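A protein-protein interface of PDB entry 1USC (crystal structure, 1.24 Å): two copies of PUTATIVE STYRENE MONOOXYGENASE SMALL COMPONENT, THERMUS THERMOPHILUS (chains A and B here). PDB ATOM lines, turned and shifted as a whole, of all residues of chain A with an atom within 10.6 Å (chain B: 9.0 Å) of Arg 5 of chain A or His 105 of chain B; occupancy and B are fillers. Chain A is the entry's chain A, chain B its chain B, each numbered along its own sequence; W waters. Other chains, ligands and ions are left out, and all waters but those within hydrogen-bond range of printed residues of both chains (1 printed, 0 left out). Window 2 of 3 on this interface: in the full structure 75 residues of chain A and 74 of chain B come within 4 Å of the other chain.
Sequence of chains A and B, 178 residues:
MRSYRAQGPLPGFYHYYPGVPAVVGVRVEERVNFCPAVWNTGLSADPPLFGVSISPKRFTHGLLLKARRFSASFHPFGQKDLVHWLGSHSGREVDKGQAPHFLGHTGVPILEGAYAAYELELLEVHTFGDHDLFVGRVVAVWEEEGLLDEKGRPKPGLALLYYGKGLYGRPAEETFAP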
ATOM      1  N   MET A   1       9.460  28.120 -10.173  1.00  0.00           N
ATOM      2  CA  MET A   1       9.926  27.409  -8.949  1.00  0.00           C
ATOM      3  C   MET A   1      10.179  25.937  -9.265  1.00  0.00           C
ATOM      4  O   MET A   1       9.252  25.187  -9.571  1.00  0.00           O
ATOM      5  CB  MET A   1       8.877  27.552  -7.839  1.00  0.00           C
ATOM      6  CG  MET A   1       9.253  26.918  -6.510  1.00  0.00           C
ATOM      7  SD  MET A   1       8.174  27.456  -5.151  1.00  0.00           S
ATOM      8  CE  MET A   1       9.369  27.526  -3.783  1.00  0.00           C
ATOM      9  N   ARG A   2      11.446  25.535  -9.200  1.00  0.00           N
ATOM     10  CA  ARG A   2      11.845  24.157  -9.480  1.00  0.00           C
ATOM     11  C   ARG A   2      11.195  23.176  -8.519  1.00  0.00           C
ATOM     12  O   ARG A   2      10.971  23.493  -7.353  1.00  0.00           O
ATOM     13  CB  ARG A   2      13.365  24.006  -9.359  1.00  0.00           C
ATOM     14  CG  ARG A   2      13.859  22.568  -9.495  1.00  0.00           C
ATOM     15  CD  ARG A   2      15.161  22.337  -8.734  1.00  0.00           C
ATOM     16  NE  ARG A   2      15.628  20.958  -8.866  1.00  0.00           N
ATOM     17  CZ  ARG A   2      16.614  20.425  -8.151  1.00  0.00           C
ATOM     18  NH1 ARG A   2      17.247  21.152  -7.239  1.00  0.00           N
ATOM     19  NH2 ARG A   2      16.975  19.164  -8.351  1.00  0.00           N
ATOM     20  N   SER A   3      10.904  21.977  -9.009  1.00  0.00           N
ATOM     21  CA  SER A   3      10.321  20.946  -8.167  1.00  0.00           C
ATOM     22  C   SER A   3      10.786  19.575  -8.622  1.00  0.00           C
ATOM     23  O   SER A   3      11.159  19.379  -9.782  1.00  0.00           O
ATOM     24  CB  SER A   3       8.791  20.995  -8.204  1.00  0.00           C
ATOM     25  OG  SER A   3       8.289  20.471  -9.419  1.00  0.00           O
ATOM     26  N   TYR A   4      10.786  18.633  -7.693  1.00  0.00           N
ATOM     27  CA  TYR A   4      11.158  17.265  -7.992  1.00  0.00           C
ATOM     28  C   TYR A   4      10.503  16.369  -6.957  1.00  0.00           C
ATOM     29  O   TYR A   4      10.209  16.805  -5.842  1.00  0.00           O
ATOM     30  CB  TYR A   4      12.691  17.092  -8.005  1.00  0.00           C
ATOM     31  CG  TYR A   4      13.412  17.288  -6.686  1.00  0.00           C
ATOM     32  CD1 TYR A   4      13.483  16.260  -5.741  1.00  0.00           C
ATOM     33  CD2 TYR A   4      14.054  18.493  -6.395  1.00  0.00           C
ATOM     34  CE1 TYR A   4      14.180  16.428  -4.541  1.00  0.00           C
ATOM     35  CE2 TYR A   4      14.752  18.671  -5.199  1.00  0.00           C
ATOM     36  CZ  TYR A   4      14.809  17.635  -4.277  1.00  0.00           C
ATOM     37  OH  TYR A   4      15.483  17.813  -3.091  1.00  0.00           O
ATOM     38  N   ARG A   5      10.230  15.128  -7.342  1.00  0.00           N
ATOM     39  CA  ARG A   5       9.613  14.177  -6.432  1.00  0.00           C
ATOM     40  C   ARG A   5      10.702  13.519  -5.602  1.00  0.00           C
ATOM     41  O   ARG A   5      11.774  13.204  -6.117  1.00  0.00           O
ATOM     42  CB  ARG A   5       8.843  13.109  -7.214  1.00  0.00           C
ATOM     43  CG  ARG A   5       7.608  13.632  -7.932  1.00  0.00           C
ATOM     44  CD  ARG A   5       6.910  12.522  -8.703  1.00  0.00           C
ATOM     45  NE  ARG A   5       5.670  12.976  -9.330  1.00  0.00           N
ATOM     46  CZ  ARG A   5       4.576  13.328  -8.661  1.00  0.00           C
ATOM     47  NH1 ARG A   5       4.560  13.280  -7.336  1.00  0.00           N
ATOM     48  NH2 ARG A   5       3.496  13.728  -9.319  1.00  0.00           N
ATOM     49  N   ALA A   6      10.437  13.330  -4.314  1.00  0.00           N
ATOM     50  CA  ALA A   6      11.406  12.694  -3.435  1.00  0.00           C
ATOM     51  C   ALA A   6      11.583  11.257  -3.901  1.00  0.00           C
ATOM     52  O   ALA A   6      10.611  10.571  -4.219  1.00  0.00           O
ATOM     53  CB  ALA A   6      10.918  12.727  -1.994  1.00  0.00           C
ATOM     54  N   GLN A   7      12.831  10.808  -3.942  1.00  0.00           N
ATOM     55  CA  GLN A   7      13.163   9.463  -4.393  1.00  0.00           C
ATOM     56  C   GLN A   7      13.993   8.753  -3.328  1.00  0.00           C
ATOM     57  O   GLN A   7      14.528   7.668  -3.551  1.00  0.00           O
ATOM     58  CB  GLN A   7      13.938   9.562  -5.712  1.00  0.00           C
ATOM     59  CG  GLN A   7      13.099  10.130  -6.859  1.00  0.00           C
ATOM     60  CD  GLN A   7      13.907  10.935  -7.866  1.00  0.00           C
ATOM     61  OE1 GLN A   7      14.871  10.440  -8.453  1.00  0.00           O
ATOM     62  NE2 GLN A   7      13.505  12.185  -8.077  1.00  0.00           N
ATOM     63  N   GLY A   8      14.066   9.384  -2.161  1.00  0.00           N
ATOM     64  CA  GLY A   8      14.826   8.859  -1.041  1.00  0.00           C
ATOM     65  C   GLY A   8      15.312  10.069  -0.268  1.00  0.00           C
ATOM     66  O   GLY A   8      14.664  11.113  -0.306  1.00  0.00           O
ATOM     67  N   PRO A   9      16.441   9.975   0.447  1.00  0.00           N
ATOM     68  CA  PRO A   9      16.918  11.147   1.191  1.00  0.00           C
ATOM     69  C   PRO A   9      17.164  12.300   0.220  1.00  0.00           C
ATOM     70  O   PRO A   9      17.551  12.078  -0.930  1.00  0.00           O
ATOM     71  CB  PRO A   9      18.221  10.648   1.826  1.00  0.00           C
ATOM     72  CG  PRO A   9      18.044   9.167   1.894  1.00  0.00           C
ATOM     73  CD  PRO A   9      17.383   8.853   0.590  1.00  0.00           C
ATOM     74  N   LEU A  10      16.931  13.527   0.669  1.00  0.00           N
ATOM     75  CA  LEU A  10      17.144  14.679  -0.196  1.00  0.00           C
ATOM     76  C   LEU A  10      18.637  14.957  -0.361  1.00  0.00           C
ATOM     77  O   LEU A  10      19.438  14.623   0.512  1.00  0.00           O
ATOM     78  CB  LEU A  10      16.450  15.917   0.385  1.00  0.00           C
ATOM     79  CG  LEU A  10      14.961  15.796   0.731  1.00  0.00           C
ATOM     80  CD1 LEU A  10      14.406  17.172   1.069  1.00  0.00           C
ATOM     81  CD2 LEU A  10      14.197  15.204  -0.443  1.00  0.00           C
ATOM     82  N   PRO A  11      19.034  15.563  -1.494  1.00  0.00           N
ATOM     83  CA  PRO A  11      20.450  15.871  -1.730  1.00  0.00           C
ATOM     84  C   PRO A  11      20.969  16.742  -0.592  1.00  0.00           C
ATOM     85  O   PRO A  11      22.120  16.630  -0.171  1.00  0.00           O
ATOM     86  CB  PRO A  11      20.422  16.620  -3.058  1.00  0.00           C
ATOM     87  CG  PRO A  11      19.263  16.003  -3.759  1.00  0.00           C
ATOM     88  CD  PRO A  11      18.220  15.911  -2.671  1.00  0.00           C
ATOM     89  N   ARG B  27      -5.523  21.196   2.365  1.00  0.00           N
ATOM     90  CA  ARG B  27      -6.727  21.308   1.554  1.00  0.00           C
ATOM     91  C   ARG B  27      -7.635  20.106   1.760  1.00  0.00           C
ATOM     92  O   ARG B  27      -7.189  18.959   1.733  1.00  0.00           O
ATOM     93  CB  ARG B  27      -6.362  21.409   0.068  1.00  0.00           C
ATOM     94  CG  ARG B  27      -7.565  21.491  -0.877  1.00  0.00           C
ATOM     95  CD  ARG B  27      -7.121  21.434  -2.332  1.00  0.00           C
ATOM     96  NE  ARG B  27      -6.603  20.115  -2.692  1.00  0.00           N
ATOM     97  CZ  ARG B  27      -7.360  19.044  -2.913  1.00  0.00           C
ATOM     98  NH1 ARG B  27      -8.681  19.128  -2.817  1.00  0.00           N
ATOM     99  NH2 ARG B  27      -6.798  17.884  -3.228  1.00  0.00           N
ATOM    100  N   PRO B  48      13.197  11.022   4.447  1.00  0.00           N
ATOM    101  CA  PRO B  48      13.067  12.425   4.849  1.00  0.00           C
ATOM    102  C   PRO B  48      11.740  12.682   5.555  1.00  0.00           C
ATOM    103  O   PRO B  48      10.679  12.651   4.929  1.00  0.00           O
ATOM    104  CB  PRO B  48      13.189  13.170   3.523  1.00  0.00           C
ATOM    105  CG  PRO B  48      12.559  12.215   2.550  1.00  0.00           C
ATOM    106  CD  PRO B  48      13.101  10.872   2.983  1.00  0.00           C
ATOM    107  N   ARG B  69      -2.422  14.826   4.206  1.00  0.00           N
ATOM    108  CA  ARG B  69      -1.415  15.379   3.304  1.00  0.00           C
ATOM    109  C   ARG B  69      -1.358  16.870   3.592  1.00  0.00           C
ATOM    110  O   ARG B  69      -2.373  17.478   3.937  1.00  0.00           O
ATOM    111  CB  ARG B  69      -1.820  15.198   1.837  1.00  0.00           C
ATOM    112  CG  ARG B  69      -1.883  13.771   1.326  1.00  0.00           C
ATOM    113  CD  ARG B  69      -2.410  13.770  -0.108  1.00  0.00           C
ATOM    114  NE  ARG B  69      -2.422  12.440  -0.711  1.00  0.00           N
ATOM    115  CZ  ARG B  69      -1.332  11.764  -1.055  1.00  0.00           C
ATOM    116  NH1 ARG B  69      -0.128  12.292  -0.860  1.00  0.00           N
ATOM    117  NH2 ARG B  69      -1.441  10.558  -1.596  1.00  0.00           N
ATOM    118  N   PHE B 102      -0.574  27.944  -4.937  1.00  0.00           N
ATOM    119  CA  PHE B 102      -0.705  27.026  -6.058  1.00  0.00           C
ATOM    120  C   PHE B 102      -0.778  25.624  -5.467  1.00  0.00           C
ATOM    121  O   PHE B 102      -0.469  25.431  -4.291  1.00  0.00           O
ATOM    122  CB  PHE B 102       0.479  27.172  -7.028  1.00  0.00           C
ATOM    123  CG  PHE B 102       1.809  26.744  -6.462  1.00  0.00           C
ATOM    124  CD1 PHE B 102       2.239  25.420  -6.572  1.00  0.00           C
ATOM    125  CD2 PHE B 102       2.647  27.671  -5.853  1.00  0.00           C
ATOM    126  CE1 PHE B 102       3.490  25.031  -6.086  1.00  0.00           C
ATOM    127  CE2 PHE B 102       3.899  27.292  -5.365  1.00  0.00           C
ATOM    128  CZ  PHE B 102       4.320  25.970  -5.483  1.00  0.00           C
ATOM    129  N   LEU B 103      -1.221  24.655  -6.260  1.00  0.00           N
ATOM    130  CA  LEU B 103      -1.325  23.285  -5.781  1.00  0.00           C
ATOM    131  C   LEU B 103      -0.123  22.478  -6.249  1.00  0.00           C
ATOM    132  O   LEU B 103       0.292  22.578  -7.403  1.00  0.00           O
ATOM    133  CB  LEU B 103      -2.619  22.637  -6.285  1.00  0.00           C
ATOM    134  CG  LEU B 103      -3.921  23.296  -5.820  1.00  0.00           C
ATOM    135  CD1 LEU B 103      -5.107  22.522  -6.372  1.00  0.00           C
ATOM    136  CD2 LEU B 103      -3.971  23.334  -4.300  1.00  0.00           C
ATOM    137  N   GLY B 104       0.437  21.688  -5.340  1.00  0.00           N
ATOM    138  CA  GLY B 104       1.586  20.869  -5.678  1.00  0.00           C
ATOM    139  C   GLY B 104       1.205  19.600  -6.416  1.00  0.00           C
ATOM    140  O   GLY B 104       0.034  19.368  -6.725  1.00  0.00           O
ATOM    141  N   HIS B 105       2.201  18.769  -6.694  1.00  0.00           N
ATOM    142  CA  HIS B 105       1.983  17.516  -7.407  1.00  0.00           C
ATOM    143  C   HIS B 105       0.984  16.593  -6.718  1.00  0.00           C
ATOM    144  O   HIS B 105       0.273  15.834  -7.379  1.00  0.00           O
ATOM    145  CB  HIS B 105       3.317  16.792  -7.587  1.00  0.00           C
ATOM    146  CG  HIS B 105       4.336  17.590  -8.339  1.00  0.00           C
ATOM    147  ND1 HIS B 105       4.178  17.938  -9.663  1.00  0.00           N
ATOM    148  CD2 HIS B 105       5.516  18.125  -7.947  1.00  0.00           C
ATOM    149  CE1 HIS B 105       5.216  18.654 -10.055  1.00  0.00           C
ATOM    150  NE2 HIS B 105       6.043  18.783  -9.033  1.00  0.00           N
ATOM    151  N   THR B 106       0.922  16.660  -5.391  1.00  0.00           N
ATOM    152  CA  THR B 106       0.013  15.809  -4.633  1.00  0.00           C
ATOM    153  C   THR B 106      -1.292  16.507  -4.272  1.00  0.00           C
ATOM    154  O   THR B 106      -2.116  15.958  -3.540  1.00  0.00           O
ATOM    155  CB  THR B 106       0.675  15.302  -3.339  1.00  0.00           C
ATOM    156  OG1 THR B 106       0.963  16.413  -2.482  1.00  0.00           O
ATOM    157  CG2 THR B 106       1.964  14.562  -3.664  1.00  0.00           C
ATOM    158  N   GLY B 107      -1.474  17.721  -4.779  1.00  0.00           N
ATOM    159  CA  GLY B 107      -2.698  18.454  -4.514  1.00  0.00           C
ATOM    160  C   GLY B 107      -2.697  19.329  -3.276  1.00  0.00           C
ATOM    161  O   GLY B 107      -3.699  19.984  -2.982  1.00  0.00           O
ATOM    162  N   VAL B 108      -1.595  19.338  -2.535  1.00  0.00           N
ATOM    163  CA  VAL B 108      -1.526  20.169  -1.341  1.00  0.00           C
ATOM    164  C   VAL B 108      -1.300  21.622  -1.750  1.00  0.00           C
ATOM    165  O   VAL B 108      -0.605  21.906  -2.725  1.00  0.00           O
ATOM    166  CB  VAL B 108      -0.389  19.712  -0.387  1.00  0.00           C
ATOM    167  CG1 VAL B 108      -0.670  18.301   0.103  1.00  0.00           C
ATOM    168  CG2 VAL B 108       0.961  19.779  -1.092  1.00  0.00           C
ATOM    169  N   PRO B 109      -1.906  22.565  -1.018  1.00  0.00           N
ATOM    170  CA  PRO B 109      -1.752  23.986  -1.335  1.00  0.00           C
ATOM    171  C   PRO B 109      -0.434  24.540  -0.804  1.00  0.00           C
ATOM    172  O   PRO B 109      -0.071  24.302   0.346  1.00  0.00           O
ATOM    173  CB  PRO B 109      -2.963  24.614  -0.659  1.00  0.00           C
ATOM    174  CG  PRO B 109      -3.077  23.799   0.590  1.00  0.00           C
ATOM    175  CD  PRO B 109      -2.842  22.373   0.105  1.00  0.00           C
ATOM    176  N   ILE B 110       0.275  25.279  -1.649  1.00  0.00           N
ATOM    177  CA  ILE B 110       1.557  25.866  -1.281  1.00  0.00           C
ATOM    178  C   ILE B 110       1.475  27.385  -1.407  1.00  0.00           C
ATOM    179  O   ILE B 110       1.187  27.917  -2.480  1.00  0.00           O
ATOM    180  CB  ILE B 110       2.685  25.329  -2.196  1.00  0.00           C
ATOM    181  CG1 ILE B 110       2.769  23.805  -2.064  1.00  0.00           C
ATOM    182  CG2 ILE B 110       4.015  25.987  -1.842  1.00  0.00           C
ATOM    183  CD1 ILE B 110       3.680  23.148  -3.090  1.00  0.00           C
ATOM    184  N   ALA B 117       9.729  24.704  -0.325  1.00  0.00           N
ATOM    185  CA  ALA B 117       8.548  24.084   0.256  1.00  0.00           C
ATOM    186  C   ALA B 117       8.565  22.571   0.080  1.00  0.00           C
ATOM    187  O   ALA B 117       9.162  22.048  -0.864  1.00  0.00           O
ATOM    188  CB  ALA B 117       7.286  24.668  -0.376  1.00  0.00           C
ATOM    189  N   TYR B 118       7.919  21.876   1.007  1.00  0.00           N
ATOM    190  CA  TYR B 118       7.816  20.425   0.962  1.00  0.00           C
ATOM    191  C   TYR B 118       6.354  20.022   0.827  1.00  0.00           C
ATOM    192  O   TYR B 118       5.468  20.688   1.366  1.00  0.00           O
ATOM    193  CB  TYR B 118       8.316  19.785   2.262  1.00  0.00           C
ATOM    194  CG  TYR B 118       9.778  19.950   2.600  1.00  0.00           C
ATOM    195  CD1 TYR B 118      10.188  19.986   3.932  1.00  0.00           C
ATOM    196  CD2 TYR B 118      10.754  20.027   1.606  1.00  0.00           C
ATOM    197  CE1 TYR B 118      11.522  20.094   4.269  1.00  0.00           C
ATOM    198  CE2 TYR B 118      12.104  20.130   1.934  1.00  0.00           C
ATOM    199  CZ  TYR B 118      12.475  20.163   3.272  1.00  0.00           C
ATOM    200  OH  TYR B 118      13.801  20.255   3.622  1.00  0.00           O
ATOM    201  N   GLU B 119       6.112  18.947   0.085  1.00  0.00           N
ATOM    202  CA  GLU B 119       4.785  18.373  -0.032  1.00  0.00           C
ATOM    203  C   GLU B 119       4.958  17.151   0.860  1.00  0.00           C
ATOM    204  O   GLU B 119       5.902  16.377   0.678  1.00  0.00           O
ATOM    205  CB  GLU B 119       4.483  17.955  -1.470  1.00  0.00           C
ATOM    206  CG  GLU B 119       4.329  19.124  -2.422  1.00  0.00           C
ATOM    207  CD  GLU B 119       3.714  18.717  -3.746  1.00  0.00           C
ATOM    208  OE1 GLU B 119       2.660  18.049  -3.724  1.00  0.00           O
ATOM    209  OE2 GLU B 119       4.275  19.076  -4.804  1.00  0.00           O
ATOM    210  N   LEU B 120       4.071  16.982   1.834  1.00  0.00           N
ATOM    211  CA  LEU B 120       4.197  15.866   2.760  1.00  0.00           C
ATOM    212  C   LEU B 120       2.990  14.956   2.857  1.00  0.00           C
ATOM    213  O   LEU B 120       1.848  15.382   2.671  1.00  0.00           O
ATOM    214  CB  LEU B 120       4.524  16.388   4.164  1.00  0.00           C
ATOM    215  CG  LEU B 120       5.759  17.284   4.277  1.00  0.00           C
ATOM    216  CD1 LEU B 120       5.326  18.733   4.421  1.00  0.00           C
ATOM    217  CD2 LEU B 120       6.596  16.858   5.470  1.00  0.00           C
ATOM    218  N   VAL B 138       8.445  13.608   3.375  1.00  0.00           N
ATOM    219  CA  VAL B 138       8.598  14.500   2.234  1.00  0.00           C
ATOM    220  C   VAL B 138       8.470  13.702   0.938  1.00  0.00           C
ATOM    221  O   VAL B 138       9.259  12.786   0.690  1.00  0.00           O
ATOM    222  CB  VAL B 138       9.974  15.210   2.252  1.00  0.00           C
ATOM    223  CG1 VAL B 138      10.117  16.109   1.027  1.00  0.00           C
ATOM    224  CG2 VAL B 138      10.122  16.029   3.530  1.00  0.00           C
ATOM    225  N   VAL B 139       7.476  14.042   0.121  1.00  0.00           N
ATOM    226  CA  VAL B 139       7.271  13.340  -1.146  1.00  0.00           C
ATOM    227  C   VAL B 139       7.598  14.201  -2.365  1.00  0.00           C
ATOM    228  O   VAL B 139       7.746  13.688  -3.474  1.00  0.00           O
ATOM    229  CB  VAL B 139       5.824  12.809  -1.267  1.00  0.00           C
ATOM    230  CG1 VAL B 139       5.559  11.787  -0.174  1.00  0.00           C
ATOM    231  CG2 VAL B 139       4.832  13.953  -1.174  1.00  0.00           C
ATOM    232  N   ALA B 140       7.703  15.509  -2.162  1.00  0.00           N
ATOM    233  CA  ALA B 140       8.048  16.424  -3.241  1.00  0.00           C
ATOM    234  C   ALA B 140       8.698  17.667  -2.651  1.00  0.00           C
ATOM    235  O   ALA B 140       8.377  18.082  -1.532  1.00  0.00           O
ATOM    236  CB  ALA B 140       6.806  16.798  -4.051  1.00  0.00           C
ATOM    237  N   VAL B 141       9.614  18.252  -3.412  1.00  0.00           N
ATOM    238  CA  VAL B 141      10.352  19.431  -2.986  1.00  0.00           C
ATOM    239  C   VAL B 141      10.260  20.553  -4.012  1.00  0.00           C
ATOM    240  O   VAL B 141      10.377  20.316  -5.211  1.00  0.00           O
ATOM    241  CB  VAL B 141      11.844  19.086  -2.774  1.00  0.00           C
ATOM    242  CG1 VAL B 141      12.602  20.308  -2.288  1.00  0.00           C
ATOM    243  CG2 VAL B 141      11.976  17.941  -1.788  1.00  0.00           C
ATOM    244  N   TRP B 142      10.041  21.769  -3.526  1.00  0.00           N
ATOM    245  CA  TRP B 142       9.961  22.950  -4.376  1.00  0.00           C
ATOM    246  C   TRP B 142      11.060  23.912  -3.946  1.00  0.00           C
ATOM    247  O   TRP B 142      11.293  24.100  -2.751  1.00  0.00           O
ATOM    248  CB  TRP B 142       8.593  23.629  -4.235  1.00  0.00           C
ATOM    249  CG  TRP B 142       7.471  22.820  -4.797  1.00  0.00           C
ATOM    250  CD1 TRP B 142       6.851  21.757  -4.212  1.00  0.00           C
ATOM    251  CD2 TRP B 142       6.874  22.972  -6.091  1.00  0.00           C
ATOM    252  NE1 TRP B 142       5.904  21.233  -5.061  1.00  0.00           N
ATOM    253  CE2 TRP B 142       5.899  21.959  -6.222  1.00  0.00           C
ATOM    254  CE3 TRP B 142       7.074  23.863  -7.155  1.00  0.00           C
ATOM    255  CZ2 TRP B 142       5.121  21.812  -7.376  1.00  0.00           C
ATOM    256  CZ3 TRP B 142       6.299  23.715  -8.305  1.00  0.00           C
ATOM    257  CH2 TRP B 142       5.336  22.696  -8.403  1.00  0.00           C
HETATM  258  O   HOH W   1       8.005  10.979  -3.774  1.00  0.00           O
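The side-chain hydroxyl (OG) of Ser 3 of chain A sits at hydrogen-bond distance from a ring nitrogen (NE2) of His 105 of chain B, 2.8 Å away. The backbone NH (N) of Val 141 of chain B is in hydrogen-bond range of the backbone carbonyl oxygen (O) of Tyr 4 of chain A (2.9 Å). The backbone carbonyl oxygen (O) of Val 139 of chain B sits at hydrogen-bond distance from the backbone NH (N) of Ala 6 of chain A.
The backbone carbonyl oxygen (O) of Pro 48 of chain B sits at hydrogen-bond distance from the backbone NH (N) of Val 138 of chain B (2.9 Å). The side-chain carboxylate (OE2) of Glu 119 of chain B is in hydrogen-bond range of the backbone NH (N) of His 105 of chain B, 2.8 Å away. N of Trp 142 of chain B sits at hydrogen-bond distance from O of Ala 117 of chain B, 2.8 Å away. O of Glu 119 of chain B sits at hydrogen-bond distance from N of Val 139 of chain B, at 2.9 Å. The backbone NH of Glu 119 of chain B sits at hydrogen-bond distance from the backbone carbonyl oxygen of Ala 140 of chain B (2.9 Å). OE2 of Glu 119 of chain B sits at hydrogen-bond distance from NE1 of Trp 142 of chain B (2.7 Å).
Among the printed residues, pairs that only touch across the chains: Ser 3 of chain A with Val 141 of chain B (3.0 Å), Ala 6 of chain A with Val 138 of chain B (3.2 Å), Arg 2 of chain A with Trp 142 of chain B (3.2 Å), Tyr 4 of chain A with Ala 140 of chain B (3.4 Å), Ser 3 of chain A with Trp 142 of chain B (3.5 Å), Met 1 of chain A with Trp 142 of chain B (3.5 Å), Arg 5 of chain A with His 105 of chain B (3.5 Å), Arg 5 of chain A with Val 139 of chain B (3.5 Å), Gly 8 of chain A with Pro 48 of chain B (3.6 Å), Leu 10 of chain A with Val 141 of chain B (3.8 Å), Leu 10 of chain A with Tyr 118 of chain B (3.8 Å) and Arg 2 of chain A with Val 141 of chain B (3.9 Å).
Printed residues of chain B within 4 Å of Arg 5 of chain A: His 105 (3.5 Å) and Val 139 (3.5 Å). Of the printed residues of chain B, Ala 6 of chain A touches Val 138 and Val 139. Printed residues of chain B within 4 Å of Gly 8 of chain A: Pro 48 (3.6 Å). Of the printed residues of chain A, Pro 48 of chain B touches Gly 8 (3.6 Å). Leu 103 of chain B touches none of the printed residues of chain A. No residue of chain A comes within 4 Å of Gly 104 of chain B. Of chain A, only Ser 3 (2.8 Å) and Arg 5 (3.5 Å) come within 4 Å of His 105 of chain B. No residue of chain A comes within 4 Å of Thr 106 of chain B. Pro 109 of chain B touches none of the printed residues of chain A. Of the printed residues of chain A, Tyr 118 of chain B touches Leu 10. Of the printed residues of chain A, Val 139 of chain B touches Arg 5 (3.5 Å) and Ala 6 (2.8 Å). Of the printed residues of chain A, Val 141 of chain B touches Arg 2, Ser 3, Tyr 4 and Leu 10. The nearest residue of chain B that does not touch Arg 5 of chain A is Ala 140 of chain B (4.2 Å).
Of the 21 printed residues of chain B, 8 touch a printed residue of chain A. Printed residues of chain B that touch a printed residue of chain A: Pro 48, His 105, Tyr 118, Val 138, Val 139, Ala 140, Val 141 and Trp 142. Hydrophobic or aromatic side chains of chain B that line the printed part of chain A: Pro 48, His 105, Tyr 118, Ala 140, Val 141 and Trp 142. Of the 11 printed residues of chain A, 8 touch a printed residue of chain B.
No position is printed for both chains.
Water W1 lies within hydrogen-bond range of the backbone carbonyl oxygen (O) of Ala 6 of chain A (2.7 Å) and the backbone carbonyl oxygen (O) of Val 139 of chain B (2.7 Å).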
